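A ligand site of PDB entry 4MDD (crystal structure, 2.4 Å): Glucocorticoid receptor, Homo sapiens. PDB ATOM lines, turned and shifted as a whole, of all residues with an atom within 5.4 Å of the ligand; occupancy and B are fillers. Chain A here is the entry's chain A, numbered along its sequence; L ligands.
The side-chain amide oxygen (OD1) of Asn 45 lies within hydrogen-bond range of a nitrogen (N1) of the ligand (3.1 Å).
A nitrogen (N3) of the ligand lies within hydrogen-bond range of the backbone carbonyl oxygen (O) of Met 41 (3.2 Å).
ND2 of Asn 45 sits close to O of Met 41, 3.1 Å away.
The side-chain hydroxyl (OG1) of Thr 220 is in hydrogen-bond range of the backbone carbonyl oxygen (O) of Tyr 216 (2.7 Å).
SG of Cys 217 lies close to O of Leu 213 (3.5 Å).
The backbone carbonyl oxygen of Met 120 lies within hydrogen-bond range of the side-chain sulfur of Cys 124.
The side-chain sulfur (SG) of Cys 124 is in hydrogen-bond range of the side-chain sulfur (SD) of Met 115 (3.3 Å).
The backbone carbonyl oxygen (O) of Leu 44 lies close to an oxygen (O1) of the ligand.
F1 of the ligand sits close to O of Met 85, 3.0 Å away.
A fluorine (F1) of the ligand lies close to the backbone NH of Ala 86, 3.4 Å away.
Merely in contact with the ligand: Thr 220 (3.3 Å), Cys 217 (3.5 Å), Leu 89 (3.6 Å), Gln 51 (3.6 Å), Trp 81 (3.7 Å), Met 82 (3.7 Å), Phe 104 (3.7 Å), Gly 48 (3.7 Å), Met 120 (3.7 Å), Tyr 216 (3.7 Å), Met 115 (3.8 Å), Leu 214 (3.9 Å), Met 127 (3.9 Å), Phe 221 (3.9 Å), Phe 218 (3.9 Å) and Leu 47 (3.96 Å).
The nearest printed residue that does not touch the ligand is Leu 213 (4.1 Å).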
ATOM      1  N   ILE A  40      13.822  12.362 -23.734  1.00  0.00           N
ATOM      2  CA  ILE A  40      14.644  12.712 -22.574  1.00  0.00           C
ATOM      3  C   ILE A  40      14.418  11.720 -21.427  1.00  0.00           C
ATOM      4  O   ILE A  40      15.401  11.198 -20.888  1.00  0.00           O
ATOM      5  CB  ILE A  40      14.437  14.203 -22.174  1.00  0.00           C
ATOM      6  CG1 ILE A  40      15.078  15.135 -23.223  1.00  0.00           C
ATOM      7  CG2 ILE A  40      14.928  14.507 -20.750  1.00  0.00           C
ATOM      8  CD1 ILE A  40      14.495  16.582 -23.317  1.00  0.00           C
ATOM      9  N   MET A  41      13.152  11.398 -21.105  1.00  0.00           N
ATOM     10  CA  MET A  41      12.917  10.546 -19.944  1.00  0.00           C
ATOM     11  C   MET A  41      13.268   9.043 -20.202  1.00  0.00           C
ATOM     12  O   MET A  41      13.805   8.434 -19.280  1.00  0.00           O
ATOM     13  CB  MET A  41      11.544  10.758 -19.286  1.00  0.00           C
ATOM     14  CG  MET A  41      10.352  10.353 -20.027  1.00  0.00           C
ATOM     15  SD  MET A  41       8.831  10.796 -19.130  1.00  0.00           S
ATOM     16  CE  MET A  41       7.659  10.180 -20.307  1.00  0.00           C
ATOM     17  N   THR A  42      13.190   8.537 -21.457  1.00  0.00           N
ATOM     18  CA  THR A  42      13.622   7.182 -21.844  1.00  0.00           C
ATOM     19  C   THR A  42      15.163   7.142 -21.920  1.00  0.00           C
ATOM     20  O   THR A  42      15.766   6.138 -21.511  1.00  0.00           O
ATOM     21  CB  THR A  42      12.968   6.790 -23.193  1.00  0.00           C
ATOM     22  OG1 THR A  42      11.556   6.970 -23.097  1.00  0.00           O
ATOM     23  CG2 THR A  42      13.283   5.357 -23.614  1.00  0.00           C
ATOM     24  N   LEU A  44      17.243   9.164 -20.207  1.00  0.00           N
ATOM     25  CA  LEU A  44      17.771   9.206 -18.849  1.00  0.00           C
ATOM     26  C   LEU A  44      17.646   7.855 -18.140  1.00  0.00           C
ATOM     27  O   LEU A  44      18.606   7.472 -17.464  1.00  0.00           O
ATOM     28  CB  LEU A  44      17.228  10.369 -18.020  1.00  0.00           C
ATOM     29  CG  LEU A  44      17.730  11.756 -18.491  1.00  0.00           C
ATOM     30  CD1 LEU A  44      16.896  12.882 -17.908  1.00  0.00           C
ATOM     31  CD2 LEU A  44      19.181  11.936 -18.158  1.00  0.00           C
ATOM     32  N   ASN A  45      16.542   7.081 -18.378  1.00  0.00           N
ATOM     33  CA  ASN A  45      16.403   5.745 -17.768  1.00  0.00           C
ATOM     34  C   ASN A  45      17.499   4.775 -18.171  1.00  0.00           C
ATOM     35  O   ASN A  45      18.006   4.032 -17.317  1.00  0.00           O
ATOM     36  CB  ASN A  45      15.053   5.110 -18.058  1.00  0.00           C
ATOM     37  CG  ASN A  45      13.915   5.894 -17.503  1.00  0.00           C
ATOM     38  OD1 ASN A  45      14.048   6.702 -16.578  1.00  0.00           O
ATOM     39  ND2 ASN A  45      12.766   5.712 -18.113  1.00  0.00           N
ATOM     40  N   LEU A  47      20.602   5.655 -19.488  1.00  0.00           N
ATOM     41  CA  LEU A  47      21.845   6.216 -18.956  1.00  0.00           C
ATOM     42  C   LEU A  47      22.032   5.880 -17.456  1.00  0.00           C
ATOM     43  O   LEU A  47      23.147   5.530 -17.035  1.00  0.00           O
ATOM     44  CB  LEU A  47      21.911   7.730 -19.229  1.00  0.00           C
ATOM     45  CG  LEU A  47      23.094   8.523 -18.595  1.00  0.00           C
ATOM     46  CD1 LEU A  47      24.454   7.980 -19.056  1.00  0.00           C
ATOM     47  CD2 LEU A  47      22.975  10.032 -18.872  1.00  0.00           C
ATOM     48  N   GLY A  48      20.943   5.968 -16.682  1.00  0.00           N
ATOM     49  CA  GLY A  48      20.931   5.643 -15.264  1.00  0.00           C
ATOM     50  C   GLY A  48      21.284   4.185 -15.020  1.00  0.00           C
ATOM     51  O   GLY A  48      21.958   3.875 -14.043  1.00  0.00           O
ATOM     52  N   GLY A  49      20.826   3.290 -15.906  1.00  0.00           N
ATOM     53  CA  GLY A  49      21.140   1.865 -15.825  1.00  0.00           C
ATOM     54  C   GLY A  49      22.631   1.611 -15.966  1.00  0.00           C
ATOM     55  O   GLY A  49      23.214   0.812 -15.225  1.00  0.00           O
ATOM     56  N   GLN A  51      24.976   4.092 -15.473  1.00  0.00           N
ATOM     57  CA  GLN A  51      25.549   4.822 -14.328  1.00  0.00           C
ATOM     58  C   GLN A  51      25.594   3.948 -13.073  1.00  0.00           C
ATOM     59  O   GLN A  51      26.573   4.030 -12.333  1.00  0.00           O
ATOM     60  CB  GLN A  51      24.801   6.131 -14.046  1.00  0.00           C
ATOM     61  CG  GLN A  51      25.236   7.282 -14.965  1.00  0.00           C
ATOM     62  CD  GLN A  51      24.604   8.618 -14.630  1.00  0.00           C
ATOM     63  OE1 GLN A  51      23.994   8.841 -13.580  1.00  0.00           O
ATOM     64  NE2 GLN A  51      24.815   9.577 -15.496  1.00  0.00           N
ATOM     65  N   TRP A  81      22.917   3.651  -4.753  1.00  0.00           N
ATOM     66  CA  TRP A  81      23.066   3.970  -6.174  1.00  0.00           C
ATOM     67  C   TRP A  81      22.573   5.396  -6.569  1.00  0.00           C
ATOM     68  O   TRP A  81      23.321   6.116  -7.246  1.00  0.00           O
ATOM     69  CB  TRP A  81      22.387   2.894  -7.047  1.00  0.00           C
ATOM     70  CG  TRP A  81      20.887   2.819  -6.948  1.00  0.00           C
ATOM     71  CD1 TRP A  81      20.163   2.114  -6.026  1.00  0.00           C
ATOM     72  CD2 TRP A  81      19.927   3.418  -7.832  1.00  0.00           C
ATOM     73  NE1 TRP A  81      18.813   2.307  -6.234  1.00  0.00           N
ATOM     74  CE2 TRP A  81      18.644   3.085  -7.347  1.00  0.00           C
ATOM     75  CE3 TRP A  81      20.031   4.237  -8.969  1.00  0.00           C
ATOM     76  CZ2 TRP A  81      17.470   3.498  -7.992  1.00  0.00           C
ATOM     77  CZ3 TRP A  81      18.868   4.651  -9.606  1.00  0.00           C
ATOM     78  CH2 TRP A  81      17.613   4.277  -9.126  1.00  0.00           C
ATOM     79  N   MET A  82      21.394   5.826  -6.093  1.00  0.00           N
ATOM     80  CA  MET A  82      20.856   7.135  -6.481  1.00  0.00           C
ATOM     81  C   MET A  82      21.491   8.291  -5.668  1.00  0.00           C
ATOM     82  O   MET A  82      21.547   9.414  -6.171  1.00  0.00           O
ATOM     83  CB  MET A  82      19.311   7.165  -6.481  1.00  0.00           C
ATOM     84  CG  MET A  82      18.674   8.494  -6.953  1.00  0.00           C
ATOM     85  SD  MET A  82      19.237   9.099  -8.572  1.00  0.00           S
ATOM     86  CE  MET A  82      18.153   8.215  -9.682  1.00  0.00           C
ATOM     87  N   MET A  85      24.561   8.816  -7.855  1.00  0.00           N
ATOM     88  CA  MET A  85      24.168   9.430  -9.119  1.00  0.00           C
ATOM     89  C   MET A  85      23.703  10.858  -8.944  1.00  0.00           C
ATOM     90  O   MET A  85      24.185  11.719  -9.682  1.00  0.00           O
ATOM     91  CB  MET A  85      23.128   8.585  -9.860  1.00  0.00           C
ATOM     92  CG  MET A  85      23.741   7.359 -10.514  1.00  0.00           C
ATOM     93  SD  MET A  85      22.571   6.023 -10.929  1.00  0.00           S
ATOM     94  CE  MET A  85      21.274   6.943 -11.797  1.00  0.00           C
ATOM     95  N   ALA A  86      22.811  11.126  -7.976  1.00  0.00           N
ATOM     96  CA  ALA A  86      22.338  12.481  -7.745  1.00  0.00           C
ATOM     97  C   ALA A  86      23.464  13.430  -7.272  1.00  0.00           C
ATOM     98  O   ALA A  86      23.456  14.583  -7.673  1.00  0.00           O
ATOM     99  CB  ALA A  86      21.157  12.504  -6.783  1.00  0.00           C
ATOM    100  N   LEU A  89      25.727  14.120 -10.370  1.00  0.00           N
ATOM    101  CA  LEU A  89      24.961  15.023 -11.214  1.00  0.00           C
ATOM    102  C   LEU A  89      25.134  16.475 -10.686  1.00  0.00           C
ATOM    103  O   LEU A  89      25.357  17.385 -11.466  1.00  0.00           O
ATOM    104  CB  LEU A  89      23.471  14.642 -11.245  1.00  0.00           C
ATOM    105  CG  LEU A  89      22.502  15.665 -11.879  1.00  0.00           C
ATOM    106  CD1 LEU A  89      22.781  15.874 -13.370  1.00  0.00           C
ATOM    107  CD2 LEU A  89      21.053  15.312 -11.617  1.00  0.00           C
ATOM    108  N   PHE A 104      23.548  16.043 -17.052  1.00  0.00           N
ATOM    109  CA  PHE A 104      23.463  14.586 -16.913  1.00  0.00           C
ATOM    110  C   PHE A 104      24.625  13.888 -17.607  1.00  0.00           C
ATOM    111  O   PHE A 104      25.174  12.913 -17.074  1.00  0.00           O
ATOM    112  CB  PHE A 104      22.116  14.064 -17.447  1.00  0.00           C
ATOM    113  CG  PHE A 104      20.934  14.384 -16.552  1.00  0.00           C
ATOM    114  CD1 PHE A 104      20.076  15.425 -16.867  1.00  0.00           C
ATOM    115  CD2 PHE A 104      20.655  13.613 -15.428  1.00  0.00           C
ATOM    116  CE1 PHE A 104      18.946  15.684 -16.089  1.00  0.00           C
ATOM    117  CE2 PHE A 104      19.554  13.893 -14.622  1.00  0.00           C
ATOM    118  CZ  PHE A 104      18.699  14.915 -14.962  1.00  0.00           C
ATOM    119  N   MET A 115      11.130  22.992 -20.013  1.00  0.00           N
ATOM    120  CA  MET A 115      10.533  21.777 -19.456  1.00  0.00           C
ATOM    121  C   MET A 115       9.026  21.989 -19.311  1.00  0.00           C
ATOM    122  O   MET A 115       8.572  22.961 -18.696  1.00  0.00           O
ATOM    123  CB  MET A 115      11.178  21.454 -18.100  1.00  0.00           C
ATOM    124  CG  MET A 115      10.953  20.035 -17.647  1.00  0.00           C
ATOM    125  SD  MET A 115      12.253  19.542 -16.499  1.00  0.00           S
ATOM    126  CE  MET A 115      13.099  18.356 -17.486  1.00  0.00           C
ATOM    127  N   MET A 120       8.264  17.745 -12.744  1.00  0.00           N
ATOM    128  CA  MET A 120       9.567  17.521 -13.367  1.00  0.00           C
ATOM    129  C   MET A 120      10.444  18.708 -12.931  1.00  0.00           C
ATOM    130  O   MET A 120      11.525  18.495 -12.383  1.00  0.00           O
ATOM    131  CB  MET A 120       9.405  17.477 -14.909  1.00  0.00           C
ATOM    132  CG  MET A 120      10.349  16.520 -15.628  1.00  0.00           C
ATOM    133  SD  MET A 120       9.680  16.003 -17.230  1.00  0.00           S
ATOM    134  CE  MET A 120      11.092  15.309 -17.980  1.00  0.00           C
ATOM    135  N   GLN A 123      11.642  18.848  -9.197  1.00  0.00           N
ATOM    136  CA  GLN A 123      12.663  17.808  -9.048  1.00  0.00           C
ATOM    137  C   GLN A 123      13.966  18.303  -9.620  1.00  0.00           C
ATOM    138  O   GLN A 123      15.036  18.061  -9.028  1.00  0.00           O
ATOM    139  CB  GLN A 123      12.213  16.524  -9.755  1.00  0.00           C
ATOM    140  CG  GLN A 123      11.782  15.413  -8.812  1.00  0.00           C
ATOM    141  CD  GLN A 123      10.798  15.835  -7.761  1.00  0.00           C
ATOM    142  OE1 GLN A 123      11.069  15.735  -6.559  1.00  0.00           O
ATOM    143  NE2 GLN A 123       9.637  16.343  -8.182  1.00  0.00           N
ATOM    144  N   CYS A 124      13.886  19.006 -10.755  1.00  0.00           N
ATOM    145  CA  CYS A 124      15.042  19.614 -11.397  1.00  0.00           C
ATOM    146  C   CYS A 124      15.631  20.682 -10.476  1.00  0.00           C
ATOM    147  O   CYS A 124      16.809  20.601 -10.166  1.00  0.00           O
ATOM    148  CB  CYS A 124      14.678  20.161 -12.780  1.00  0.00           C
ATOM    149  SG  CYS A 124      14.392  18.870 -14.026  1.00  0.00           S
ATOM    150  N   MET A 127      17.379  18.819  -7.741  1.00  0.00           N
ATOM    151  CA  MET A 127      18.652  18.274  -8.218  1.00  0.00           C
ATOM    152  C   MET A 127      19.621  19.462  -8.368  1.00  0.00           C
ATOM    153  O   MET A 127      20.805  19.342  -8.037  1.00  0.00           O
ATOM    154  CB  MET A 127      18.480  17.495  -9.540  1.00  0.00           C
ATOM    155  CG  MET A 127      17.874  16.079  -9.382  1.00  0.00           C
ATOM    156  SD  MET A 127      17.496  15.178 -10.931  1.00  0.00           S
ATOM    157  CE  MET A 127      15.769  15.643 -11.239  1.00  0.00           C
ATOM    158  N   LEU A 213      13.308  12.210  -4.976  1.00  0.00           N
ATOM    159  CA  LEU A 213      13.698  11.963  -6.342  1.00  0.00           C
ATOM    160  C   LEU A 213      13.261  10.554  -6.756  1.00  0.00           C
ATOM    161  O   LEU A 213      12.615  10.413  -7.782  1.00  0.00           O
ATOM    162  CB  LEU A 213      15.222  12.179  -6.481  1.00  0.00           C
ATOM    163  CG  LEU A 213      15.918  11.839  -7.789  1.00  0.00           C
ATOM    164  CD1 LEU A 213      15.228  12.516  -9.001  1.00  0.00           C
ATOM    165  CD2 LEU A 213      17.379  12.259  -7.716  1.00  0.00           C
ATOM    166  N   LEU A 214      13.565   9.510  -5.941  1.00  0.00           N
ATOM    167  CA  LEU A 214      13.134   8.146  -6.264  1.00  0.00           C
ATOM    168  C   LEU A 214      11.604   8.018  -6.281  1.00  0.00           C
ATOM    169  O   LEU A 214      11.055   7.304  -7.123  1.00  0.00           O
ATOM    170  CB  LEU A 214      13.788   7.090  -5.354  1.00  0.00           C
ATOM    171  CG  LEU A 214      15.283   6.900  -5.662  1.00  0.00           C
ATOM    172  CD1 LEU A 214      15.923   5.922  -4.700  1.00  0.00           C
ATOM    173  CD2 LEU A 214      15.507   6.472  -7.134  1.00  0.00           C
ATOM    174  N   TYR A 216       9.374  10.483  -7.154  1.00  0.00           N
ATOM    175  CA  TYR A 216       9.000  11.090  -8.416  1.00  0.00           C
ATOM    176  C   TYR A 216       9.355  10.178  -9.587  1.00  0.00           C
ATOM    177  O   TYR A 216       8.530   9.995 -10.479  1.00  0.00           O
ATOM    178  CB  TYR A 216       9.632  12.488  -8.604  1.00  0.00           C
ATOM    179  CG  TYR A 216       9.376  13.036 -10.000  1.00  0.00           C
ATOM    180  CD1 TYR A 216      10.284  12.803 -11.039  1.00  0.00           C
ATOM    181  CD2 TYR A 216       8.186  13.691 -10.312  1.00  0.00           C
ATOM    182  CE1 TYR A 216      10.012  13.202 -12.344  1.00  0.00           C
ATOM    183  CE2 TYR A 216       7.918  14.127 -11.616  1.00  0.00           C
ATOM    184  CZ  TYR A 216       8.843  13.886 -12.619  1.00  0.00           C
ATOM    185  OH  TYR A 216       8.585  14.321 -13.901  1.00  0.00           O
ATOM    186  N   CYS A 217      10.595   9.643  -9.615  1.00  0.00           N
ATOM    187  CA  CYS A 217      11.043   8.779 -10.716  1.00  0.00           C
ATOM    188  C   CYS A 217      10.182   7.529 -10.859  1.00  0.00           C
ATOM    189  O   CYS A 217       9.704   7.238 -11.952  1.00  0.00           O
ATOM    190  CB  CYS A 217      12.526   8.430 -10.587  1.00  0.00           C
ATOM    191  SG  CYS A 217      13.654   9.772 -11.038  1.00  0.00           S
ATOM    192  N   PHE A 218       9.968   6.789  -9.744  1.00  0.00           N
ATOM    193  CA  PHE A 218       9.163   5.575  -9.744  1.00  0.00           C
ATOM    194  C   PHE A 218       7.721   5.884 -10.153  1.00  0.00           C
ATOM    195  O   PHE A 218       7.173   5.173 -11.009  1.00  0.00           O
ATOM    196  CB  PHE A 218       9.233   4.880  -8.375  1.00  0.00           C
ATOM    197  CG  PHE A 218       8.904   3.400  -8.358  1.00  0.00           C
ATOM    198  CD1 PHE A 218       7.948   2.897  -7.480  1.00  0.00           C
ATOM    199  CD2 PHE A 218       9.571   2.501  -9.192  1.00  0.00           C
ATOM    200  CE1 PHE A 218       7.658   1.519  -7.437  1.00  0.00           C
ATOM    201  CE2 PHE A 218       9.256   1.140  -9.177  1.00  0.00           C
ATOM    202  CZ  PHE A 218       8.297   0.657  -8.309  1.00  0.00           C
ATOM    203  N   THR A 220       6.485   8.561 -12.013  1.00  0.00           N
ATOM    204  CA  THR A 220       6.502   8.928 -13.421  1.00  0.00           C
ATOM    205  C   THR A 220       6.713   7.682 -14.306  1.00  0.00           C
ATOM    206  O   THR A 220       5.943   7.473 -15.242  1.00  0.00           O
ATOM    207  CB  THR A 220       7.566  10.000 -13.689  1.00  0.00           C
ATOM    208  OG1 THR A 220       7.399  11.058 -12.739  1.00  0.00           O
ATOM    209  CG2 THR A 220       7.474  10.556 -15.090  1.00  0.00           C
ATOM    210  N   PHE A 221       7.706   6.850 -13.977  1.00  0.00           N
ATOM    211  CA  PHE A 221       7.998   5.626 -14.705  1.00  0.00           C
ATOM    212  C   PHE A 221       6.777   4.694 -14.755  1.00  0.00           C
ATOM    213  O   PHE A 221       6.428   4.211 -15.835  1.00  0.00           O
ATOM    214  CB  PHE A 221       9.197   4.918 -14.069  1.00  0.00           C
ATOM    215  CG  PHE A 221       9.599   3.645 -14.768  1.00  0.00           C
ATOM    216  CD1 PHE A 221      10.267   3.675 -15.991  1.00  0.00           C
ATOM    217  CD2 PHE A 221       9.327   2.410 -14.200  1.00  0.00           C
ATOM    218  CE1 PHE A 221      10.630   2.496 -16.630  1.00  0.00           C
ATOM    219  CE2 PHE A 221       9.734   1.233 -14.826  1.00  0.00           C
ATOM    220  CZ  PHE A 221      10.379   1.288 -16.047  1.00  0.00           C
ATOM    221  N   THR A 225       5.623   5.024 -18.444  1.00  0.00           N
ATOM    222  CA  THR A 225       6.305   3.948 -19.154  1.00  0.00           C
ATOM    223  C   THR A 225       5.617   2.627 -18.904  1.00  0.00           C
ATOM    224  O   THR A 225       5.088   2.072 -19.856  1.00  0.00           O
ATOM    225  CB  THR A 225       7.829   3.927 -18.872  1.00  0.00           C
ATOM    226  OG1 THR A 225       8.375   5.181 -19.287  1.00  0.00           O
ATOM    227  CG2 THR A 225       8.560   2.808 -19.638  1.00  0.00           C
HETATM  228  C1  LIG L   1      14.526  12.853 -14.889  1.00  0.00           C
HETATM  229  F1  LIG L   1      21.526  11.633 -11.080  1.00  0.00           F
HETATM  230  N1  LIG L   1      15.574   8.951 -15.100  1.00  0.00           N
HETATM  231  O1  LIG L   1      19.588   9.618 -14.949  1.00  0.00           O
HETATM  232  S1  LIG L   1      11.596   9.191 -15.731  1.00  0.00           S
HETATM  233  C2  LIG L   1      13.666  12.032 -15.601  1.00  0.00           C
HETATM  234  N2  LIG L   1      16.651   6.485 -13.812  1.00  0.00           N
HETATM  235  O2  LIG L   1      10.934   8.322 -16.682  1.00  0.00           O
HETATM  236  C3  LIG L   1      13.900  10.670 -15.717  1.00  0.00           C
HETATM  237  N3  LIG L   1      13.035   9.781 -16.459  1.00  0.00           N
HETATM  238  O3  LIG L   1      11.835   8.652 -14.408  1.00  0.00           O
HETATM  239  C4  LIG L   1      15.058  10.215 -15.126  1.00  0.00           C
HETATM  240  C5  LIG L   1      16.751   8.902 -14.421  1.00  0.00           C
HETATM  241  C6  LIG L   1      17.022  10.191 -13.983  1.00  0.00           C
HETATM  242  C7  LIG L   1      15.951  11.012 -14.430  1.00  0.00           C
HETATM  243  C8  LIG L   1      15.682  12.363 -14.312  1.00  0.00           C
HETATM  244  C9  LIG L   1      18.213  10.567 -13.248  1.00  0.00           C
HETATM  245  C10 LIG L   1      18.065  11.237 -12.052  1.00  0.00           C
HETATM  246  C11 LIG L   1      19.177  11.604 -11.318  1.00  0.00           C
HETATM  247  C12 LIG L   1      20.444  11.289 -11.798  1.00  0.00           C
HETATM  248  C13 LIG L   1      20.609  10.636 -12.996  1.00  0.00           C
HETATM  249  C14 LIG L   1      19.489  10.276 -13.721  1.00  0.00           C
HETATM  250  C15 LIG L   1      20.936   9.484 -15.411  1.00  0.00           C
HETATM  251  C16 LIG L   1      17.476   7.627 -14.269  1.00  0.00           C
HETATM  252  C17 LIG L   1      17.377   5.202 -13.975  1.00  0.00           C
HETATM  253  C18 LIG L   1      16.133   6.677 -12.433  1.00  0.00           C
HETATM  254  C19 LIG L   1      14.888   5.886 -12.137  1.00  0.00           C
HETATM  255  C20 LIG L   1      14.049   5.442 -13.144  1.00  0.00           C
HETATM  256  C21 LIG L   1      12.908   4.723 -12.830  1.00  0.00           C
HETATM  257  C22 LIG L   1      12.599   4.460 -11.513  1.00  0.00           C
HETATM  258  C23 LIG L   1      13.437   4.900 -10.514  1.00  0.00           C
HETATM  259  C24 LIG L   1      14.581   5.599 -10.818  1.00  0.00           C
HETATM  260  C25 LIG L   1      10.728  10.714 -15.559  1.00  0.00           C
HETATM  261  C26 LIG L   1      14.315  14.326 -14.725  1.00  0.00           C
HETATM  262  C27 LIG L   1      13.091  14.650 -13.906  1.00  0.00           C
HETATM  263  C28 LIG L   1      14.297  15.017 -16.068  1.00  0.00           C
